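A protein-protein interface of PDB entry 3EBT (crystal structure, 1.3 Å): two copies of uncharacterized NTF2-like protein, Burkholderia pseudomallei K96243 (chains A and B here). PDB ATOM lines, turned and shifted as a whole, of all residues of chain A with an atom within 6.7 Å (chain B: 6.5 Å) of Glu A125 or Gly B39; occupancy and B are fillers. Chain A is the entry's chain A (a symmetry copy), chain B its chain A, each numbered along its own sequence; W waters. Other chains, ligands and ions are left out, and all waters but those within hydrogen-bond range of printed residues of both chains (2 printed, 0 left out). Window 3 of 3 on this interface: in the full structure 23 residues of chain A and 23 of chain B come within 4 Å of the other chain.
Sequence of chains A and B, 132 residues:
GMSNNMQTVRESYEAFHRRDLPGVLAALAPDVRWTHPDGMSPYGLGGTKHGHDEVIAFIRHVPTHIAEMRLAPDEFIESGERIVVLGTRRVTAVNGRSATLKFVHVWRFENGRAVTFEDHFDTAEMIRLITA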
ATOM      1  N   ALA A  99     -14.465  34.956  -5.163  1.00  0.00           N
ATOM      2  CA  ALA A  99     -13.823  34.267  -6.276  1.00  0.00           C
ATOM      3  C   ALA A  99     -14.280  34.871  -7.573  1.00  0.00           C
ATOM      4  O   ALA A  99     -15.321  35.530  -7.624  1.00  0.00           O
ATOM      5  CB  ALA A  99     -14.097  32.749  -6.273  1.00  0.00           C
ATOM      6  N   THR A 100     -13.494  34.638  -8.617  1.00  0.00           N
ATOM      7  CA  THR A 100     -13.864  35.000  -9.982  1.00  0.00           C
ATOM      8  C   THR A 100     -14.357  33.739 -10.653  1.00  0.00           C
ATOM      9  O   THR A 100     -13.686  32.717 -10.619  1.00  0.00           O
ATOM     10  CB  THR A 100     -12.713  35.622 -10.762  1.00  0.00           C
ATOM     11  OG1 THR A 100     -12.307  36.785 -10.042  1.00  0.00           O
ATOM     12  CG2 THR A 100     -13.122  36.000 -12.197  1.00  0.00           C
ATOM     13  N   LEU A 101     -15.529  33.824 -11.266  1.00  0.00           N
ATOM     14  CA  LEU A 101     -16.183  32.703 -11.910  1.00  0.00           C
ATOM     15  C   LEU A 101     -16.550  33.097 -13.340  1.00  0.00           C
ATOM     16  O   LEU A 101     -16.454  34.273 -13.713  1.00  0.00           O
ATOM     17  CB  LEU A 101     -17.434  32.330 -11.103  1.00  0.00           C
ATOM     18  CG  LEU A 101     -17.181  31.845  -9.675  1.00  0.00           C
ATOM     19  CD1 LEU A 101     -18.506  31.813  -8.873  1.00  0.00           C
ATOM     20  CD2 LEU A 101     -16.476  30.495  -9.650  1.00  0.00           C
ATOM     21  N   ASP A 122     -20.624  26.802 -13.961  1.00  0.00           N
ATOM     22  CA  ASP A 122     -20.062  25.735 -13.131  1.00  0.00           C
ATOM     23  C   ASP A 122     -20.671  25.853 -11.744  1.00  0.00           C
ATOM     24  O   ASP A 122     -20.214  26.591 -10.876  1.00  0.00           O
ATOM     25  CB  ASP A 122     -18.534  25.899 -13.126  1.00  0.00           C
ATOM     26  CG  ASP A 122     -17.770  24.762 -12.469  1.00  0.00           C
ATOM     27  OD1 ASP A 122     -18.328  24.067 -11.590  1.00  0.00           O
ATOM     28  OD2 ASP A 122     -16.569  24.636 -12.820  1.00  0.00           O
ATOM     29  N   THR A 123     -21.717  25.070 -11.543  1.00  0.00           N
ATOM     30  CA  THR A 123     -22.471  25.080 -10.305  1.00  0.00           C
ATOM     31  C   THR A 123     -21.688  24.517  -9.133  1.00  0.00           C
ATOM     32  O   THR A 123     -21.799  25.025  -8.026  1.00  0.00           O
ATOM     33  CB  THR A 123     -23.795  24.326 -10.507  1.00  0.00           C
ATOM     34  OG1 THR A 123     -23.471  23.079 -11.125  1.00  0.00           O
ATOM     35  CG2 THR A 123     -24.773  25.120 -11.380  1.00  0.00           C
ATOM     36  N   ALA A 124     -20.869  23.472  -9.353  1.00  0.00           N
ATOM     37  CA  ALA A 124     -20.024  22.953  -8.269  1.00  0.00           C
ATOM     38  C   ALA A 124     -19.117  24.060  -7.721  1.00  0.00           C
ATOM     39  O   ALA A 124     -18.957  24.210  -6.507  1.00  0.00           O
ATOM     40  CB  ALA A 124     -19.235  21.751  -8.742  1.00  0.00           C
ATOM     41  N   GLU A 125     -18.553  24.860  -8.605  1.00  0.00           N
ATOM     42  CA  GLU A 125     -17.671  25.957  -8.161  1.00  0.00           C
ATOM     43  C   GLU A 125     -18.446  27.088  -7.505  1.00  0.00           C
ATOM     44  O   GLU A 125     -17.965  27.680  -6.536  1.00  0.00           O
ATOM     45  CB  GLU A 125     -16.824  26.447  -9.326  1.00  0.00           C
ATOM     46  CG  GLU A 125     -15.741  25.459  -9.735  1.00  0.00           C
ATOM     47  CD  GLU A 125     -14.605  25.406  -8.748  1.00  0.00           C
ATOM     48  OE1 GLU A 125     -13.965  26.443  -8.577  1.00  0.00           O
ATOM     49  OE2 GLU A 125     -14.353  24.347  -8.137  1.00  0.00           O
ATOM     50  N   MET A 126     -19.658  27.390  -7.988  1.00  0.00           N
ATOM     51  CA  MET A 126     -20.483  28.413  -7.337  1.00  0.00           C
ATOM     52  C   MET A 126     -20.843  27.949  -5.926  1.00  0.00           C
ATOM     53  O   MET A 126     -20.782  28.727  -4.956  1.00  0.00           O
ATOM     54  CB  MET A 126     -21.741  28.696  -8.154  1.00  0.00           C
ATOM     55  CG  MET A 126     -22.690  29.706  -7.508  1.00  0.00           C
ATOM     56  SD  MET A 126     -22.008  31.502  -7.342  1.00  0.00           S
ATOM     57  CE  MET A 126     -22.233  31.983  -9.188  1.00  0.00           C
ATOM     58  N   ILE A 127     -21.243  26.689  -5.803  1.00  0.00           N
ATOM     59  CA  ILE A 127     -21.601  26.112  -4.503  1.00  0.00           C
ATOM     60  C   ILE A 127     -20.402  26.091  -3.554  1.00  0.00           C
ATOM     61  O   ILE A 127     -20.535  26.423  -2.375  1.00  0.00           O
ATOM     62  CB  ILE A 127     -22.278  24.738  -4.651  1.00  0.00           C
ATOM     63  CG1 ILE A 127     -23.657  24.916  -5.341  1.00  0.00           C
ATOM     64  CG2 ILE A 127     -22.438  24.028  -3.281  1.00  0.00           C
ATOM     65  CD1 ILE A 127     -24.280  23.626  -5.860  1.00  0.00           C
ATOM     66  N   ARG A 128     -19.234  25.739  -4.074  1.00  0.00           N
ATOM     67  CA  ARG A 128     -18.009  25.767  -3.260  1.00  0.00           C
ATOM     68  C   ARG A 128     -17.786  27.148  -2.656  1.00  0.00           C
ATOM     69  O   ARG A 128     -17.356  27.273  -1.512  1.00  0.00           O
ATOM     70  CB  ARG A 128     -16.835  25.345  -4.134  1.00  0.00           C
ATOM     71  CG  ARG A 128     -15.500  25.235  -3.438  1.00  0.00           C
ATOM     72  CD  ARG A 128     -14.437  24.898  -4.460  1.00  0.00           C
ATOM     73  NE  ARG A 128     -13.264  24.357  -3.842  1.00  0.00           N
ATOM     74  CZ  ARG A 128     -12.320  23.720  -4.501  1.00  0.00           C
ATOM     75  NH1 ARG A 128     -12.375  23.563  -5.831  1.00  0.00           N
ATOM     76  NH2 ARG A 128     -11.297  23.222  -3.822  1.00  0.00           N
ATOM     77  N   LEU A 129     -18.104  28.195  -3.398  1.00  0.00           N
ATOM     78  CA  LEU A 129     -17.961  29.551  -2.940  1.00  0.00           C
ATOM     79  C   LEU A 129     -18.964  29.953  -1.878  1.00  0.00           C
ATOM     80  O   LEU A 129     -18.576  30.546  -0.853  1.00  0.00           O
ATOM     81  CB  LEU A 129     -18.042  30.546  -4.082  1.00  0.00           C
ATOM     82  CG  LEU A 129     -17.905  32.029  -3.763  1.00  0.00           C
ATOM     83  CD1 LEU A 129     -16.549  32.361  -3.046  1.00  0.00           C
ATOM     84  CD2 LEU A 129     -18.091  32.880  -5.000  1.00  0.00           C
ATOM     85  N   ILE A 130     -20.243  29.632  -2.105  1.00  0.00           N
ATOM     86  CA  ILE A 130     -21.310  30.136  -1.231  1.00  0.00           C
ATOM     87  C   ILE A 130     -21.663  29.242  -0.057  1.00  0.00           C
ATOM     88  O   ILE A 130     -22.310  29.742   0.872  1.00  0.00           O
ATOM     89  CB  ILE A 130     -22.589  30.507  -2.054  1.00  0.00           C
ATOM     90  CG1 ILE A 130     -23.297  29.280  -2.649  1.00  0.00           C
ATOM     91  CG2 ILE A 130     -22.252  31.543  -3.112  1.00  0.00           C
ATOM     92  CD1 ILE A 130     -24.586  29.652  -3.379  1.00  0.00           C
ATOM     93  N   HIS B  36     -12.939  22.502 -20.413  1.00  0.00           N
ATOM     94  CA  HIS B  36     -14.068  22.011 -19.632  1.00  0.00           C
ATOM     95  C   HIS B  36     -14.046  22.624 -18.257  1.00  0.00           C
ATOM     96  O   HIS B  36     -13.022  23.186 -17.818  1.00  0.00           O
ATOM     97  CB  HIS B  36     -14.044  20.475 -19.598  1.00  0.00           C
ATOM     98  CG  HIS B  36     -14.331  19.899 -20.937  1.00  0.00           C
ATOM     99  ND1 HIS B  36     -13.378  19.815 -21.932  1.00  0.00           N
ATOM    100  CD2 HIS B  36     -15.476  19.434 -21.477  1.00  0.00           C
ATOM    101  CE1 HIS B  36     -13.927  19.316 -23.019  1.00  0.00           C
ATOM    102  NE2 HIS B  36     -15.205  19.106 -22.784  1.00  0.00           N
ATOM    103  N   PRO B  37     -15.167  22.547 -17.532  1.00  0.00           N
ATOM    104  CA  PRO B  37     -15.238  23.280 -16.271  1.00  0.00           C
ATOM    105  C   PRO B  37     -14.255  22.790 -15.219  1.00  0.00           C
ATOM    106  O   PRO B  37     -14.060  21.586 -15.055  1.00  0.00           O
ATOM    107  CB  PRO B  37     -16.684  23.053 -15.828  1.00  0.00           C
ATOM    108  CG  PRO B  37     -17.431  22.798 -17.088  1.00  0.00           C
ATOM    109  CD  PRO B  37     -16.475  21.984 -17.905  1.00  0.00           C
ATOM    110  N   ASP B  38     -13.727  23.727 -14.439  1.00  0.00           N
ATOM    111  CA  ASP B  38     -12.816  23.378 -13.340  1.00  0.00           C
ATOM    112  C   ASP B  38     -13.483  22.493 -12.295  1.00  0.00           C
ATOM    113  O   ASP B  38     -12.801  21.675 -11.668  1.00  0.00           O
ATOM    114  CB  ASP B  38     -12.136  24.609 -12.728  1.00  0.00           C
ATOM    115  CG  ASP B  38     -10.877  25.073 -13.548  1.00  0.00           C
ATOM    116  OD1 ASP B  38     -10.410  24.333 -14.439  1.00  0.00           O
ATOM    117  OD2 ASP B  38     -10.370  26.144 -13.273  1.00  0.00           O
ATOM    118  N   GLY B  39     -14.806  22.587 -12.138  1.00  0.00           N
ATOM    119  CA  GLY B  39     -15.482  21.710 -11.209  1.00  0.00           C
ATOM    120  C   GLY B  39     -15.376  20.228 -11.549  1.00  0.00           C
ATOM    121  O   GLY B  39     -15.655  19.392 -10.689  1.00  0.00           O
ATOM    122  N   MET B  40     -15.011  19.896 -12.797  1.00  0.00           N
ATOM    123  CA  MET B  40     -14.819  18.513 -13.221  1.00  0.00           C
ATOM    124  C   MET B  40     -13.433  17.973 -12.940  1.00  0.00           C
ATOM    125  O   MET B  40     -13.173  16.794 -13.192  1.00  0.00           O
ATOM    126  CB  MET B  40     -15.152  18.341 -14.691  1.00  0.00           C
ATOM    127  CG  MET B  40     -16.592  18.652 -15.035  1.00  0.00           C
ATOM    128  SD  MET B  40     -17.938  17.761 -14.011  1.00  0.00           S
ATOM    129  CE  MET B  40     -17.486  16.103 -14.315  1.00  0.00           C
ATOM    130  N   SER B  41     -12.542  18.790 -12.377  1.00  0.00           N
ATOM    131  CA  SER B  41     -11.149  18.366 -12.111  1.00  0.00           C
ATOM    132  C   SER B  41     -11.010  17.122 -11.238  1.00  0.00           C
ATOM    133  O   SER B  41     -10.104  16.327 -11.485  1.00  0.00           O
ATOM    134  CB  SER B  41     -10.288  19.523 -11.583  1.00  0.00           C
ATOM    135  OG  SER B  41     -10.683  19.953 -10.295  1.00  0.00           O
ATOM    136  N   PRO B  42     -11.893  16.922 -10.231  1.00  0.00           N
ATOM    137  CA  PRO B  42     -11.721  15.666  -9.449  1.00  0.00           C
ATOM    138  C   PRO B  42     -11.862  14.380 -10.276  1.00  0.00           C
ATOM    139  O   PRO B  42     -11.389  13.320  -9.836  1.00  0.00           O
ATOM    140  CB  PRO B  42     -12.832  15.749  -8.408  1.00  0.00           C
ATOM    141  CG  PRO B  42     -13.103  17.224  -8.251  1.00  0.00           C
ATOM    142  CD  PRO B  42     -12.963  17.755  -9.646  1.00  0.00           C
ATOM    143  N   TYR B  43     -12.534  14.456 -11.414  1.00  0.00           N
ATOM    144  CA  TYR B  43     -12.732  13.357 -12.337  1.00  0.00           C
ATOM    145  C   TYR B  43     -11.749  13.312 -13.484  1.00  0.00           C
ATOM    146  O   TYR B  43     -11.882  12.489 -14.391  1.00  0.00           O
ATOM    147  CB  TYR B  43     -14.200  13.420 -12.861  1.00  0.00           C
ATOM    148  CG  TYR B  43     -15.157  13.169 -11.740  1.00  0.00           C
ATOM    149  CD1 TYR B  43     -15.568  14.167 -10.844  1.00  0.00           C
ATOM    150  CD2 TYR B  43     -15.582  11.857 -11.494  1.00  0.00           C
ATOM    151  CE1 TYR B  43     -16.407  13.830  -9.735  1.00  0.00           C
ATOM    152  CE2 TYR B  43     -16.418  11.539 -10.453  1.00  0.00           C
ATOM    153  CZ  TYR B  43     -16.799  12.494  -9.549  1.00  0.00           C
ATOM    154  OH  TYR B  43     -17.623  12.105  -8.506  1.00  0.00           O
ATOM    155  N   GLY B  46     -11.669  18.296 -16.189  1.00  0.00           N
ATOM    156  CA  GLY B  46     -11.702  19.729 -16.133  1.00  0.00           C
ATOM    157  C   GLY B  46     -10.522  20.380 -16.805  1.00  0.00           C
ATOM    158  O   GLY B  46      -9.597  19.740 -17.283  1.00  0.00           O
ATOM    159  N   GLY B  47     -10.576  21.683 -16.844  1.00  0.00           N
ATOM    160  CA  GLY B  47      -9.467  22.517 -17.285  1.00  0.00           C
ATOM    161  C   GLY B  47      -9.294  22.654 -18.760  1.00  0.00           C
ATOM    162  O   GLY B  47     -10.140  22.244 -19.521  1.00  0.00           O
ATOM    163  N   THR B 123     -22.181  21.428 -13.537  1.00  0.00           N
ATOM    164  CA  THR B 123     -21.230  20.448 -13.051  1.00  0.00           C
ATOM    165  C   THR B 123     -21.740  19.676 -11.849  1.00  0.00           C
ATOM    166  O   THR B 123     -21.490  18.483 -11.739  1.00  0.00           O
ATOM    167  CB  THR B 123     -19.893  21.142 -12.743  1.00  0.00           C
ATOM    168  OG1 THR B 123     -20.197  22.287 -11.945  1.00  0.00           O
ATOM    169  CG2 THR B 123     -19.162  21.560 -14.024  1.00  0.00           C
ATOM    170  N   ALA B 124     -22.480  20.330 -10.935  1.00  0.00           N
ATOM    171  CA  ALA B 124     -23.072  19.603  -9.803  1.00  0.00           C
ATOM    172  C   ALA B 124     -23.973  18.472 -10.307  1.00  0.00           C
ATOM    173  O   ALA B 124     -23.936  17.351  -9.794  1.00  0.00           O
ATOM    174  CB  ALA B 124     -23.810  20.557  -8.890  1.00  0.00           C
ATOM    175  N   ILE B 127     -21.814  15.677 -11.929  1.00  0.00           N
ATOM    176  CA  ILE B 127     -21.183  14.914 -10.847  1.00  0.00           C
ATOM    177  C   ILE B 127     -22.193  14.006 -10.145  1.00  0.00           C
ATOM    178  O   ILE B 127     -21.891  12.847  -9.853  1.00  0.00           O
ATOM    179  CB  ILE B 127     -20.411  15.826  -9.877  1.00  0.00           C
ATOM    180  CG1 ILE B 127     -19.196  16.449 -10.613  1.00  0.00           C
ATOM    181  CG2 ILE B 127     -19.950  15.054  -8.612  1.00  0.00           C
ATOM    182  CD1 ILE B 127     -18.549  17.625  -9.891  1.00  0.00           C
HETATM  183  O   HOH W   1     -12.417  22.139  -8.870  1.00  0.00           O
HETATM  184  O   HOH W   2     -15.208  26.279 -14.450  1.00  0.00           O
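Printed residues of chain B that touch a printed residue of chain A: Pro B37, Asp B38, Gly B39, Thr B123 and Ala B124.
Hydrophobic or aromatic side chains of chain B that line the printed part of chain A: Pro B37 and Ala B124.
Of the 12 printed residues of chain A, 4 touch a printed residue of chain B.
Hydrophobic or aromatic side chains of chain A within 4 Å of the printed part of chain B: Ala A124.
Among the printed residues, no Asp or Glu carboxylate lies within 4 Å of a Lys or Arg side-chain nitrogen of the other chain.
Water W2 bridges the side-chain carboxylate (OD2) of Asp A122 and the backbone NH (N) of Asp B38.
Water W1 lies within hydrogen-bond range of the backbone carbonyl oxygen (O) of Asp B38 (2.9 Å), the side-chain carboxylate (OE2) of Glu A125 (3.0 Å), the side-chain hydroxyl (OG) of Ser B41 (3.1 Å) and the guanidinium group (NH1) of Arg A128 (3.4 Å).
Thr B123 touches its own counterpart, Thr A123.
Thr A123 touches Ala B124, and with the chains exchanged Ala A124 touches Thr B123.
Ala B124 touches its own counterpart, Ala A124.
Positions printed for both chains: 123, 124 and 127.
Of the 9 pairs that touch across the chains among the printed residues, 4 have their exchanged pair printed and touching as well.
The side-chain carboxylate (OD2) of Asp A122 sits at hydrogen-bond distance from the backbone NH (N) of Asp B38, 3.4 Å away.
The backbone NH (N) of Gly B39 is in hydrogen-bond range of the side-chain carboxylate (OD2) of Asp A122 (2.8 Å).
OG1 of Thr B123 is in hydrogen-bond range of OD1 of Asp A122, 2.6 Å away.
The backbone NH (N) of Thr B123 is in hydrogen-bond range of the side-chain hydroxyl (OG1) of Thr A123, 3.2 Å away.
The side-chain hydroxyl (OG1) of Thr B123 sits at hydrogen-bond distance from the backbone NH (N) of Ala A124 (2.9 Å).
The backbone NH (N) of Ala B124 lies within hydrogen-bond range of the side-chain hydroxyl (OG1) of Thr A123, 2.9 Å away.
Of the printed residues of chain B, Asp A122 touches Pro B37, Asp B38, Gly B39 and Thr B123.
Of the printed residues of chain B, Thr A123 touches Thr B123 (3.2 Å) and Ala B124 (2.9 Å).
Glu A125 touches one residue of chain B.
Of the printed residues of chain A, Asp B38 touches Asp A122.
Of the printed residues of chain A, Gly B39 touches Asp A122 (2.8 Å) and Glu A125 (3.9 Å).
The nearest printed residue of chain B that does not touch Glu A125 is Asp B38 (4.5 Å).
The nearest residue of chain A that does not touch Gly B39 is Ala A124 (4.5 Å).
The side-chain hydroxyl (OG) of Ser B41 sits at hydrogen-bond distance from the backbone carbonyl oxygen (O) of Asp B38 (3.1 Å).
N of Ala A124 lies close to OD1 of Asp A122.
The side-chain carboxylate (OD1) of Asp A122 sits at hydrogen-bond distance from the backbone NH (N) of Glu A125.
The side-chain carboxylate (OE2) of Glu A125 lies within salt-bridge range of the guanidinium group (NH1) of Arg A128 (3.1 Å).
Among the printed residues, merely in contact across the chains: Asp A122 with Pro B37 (3.4 Å), Ala A124 with Ala B124 (3.9 Å) and Glu A125 with Gly B39 (3.9 Å).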
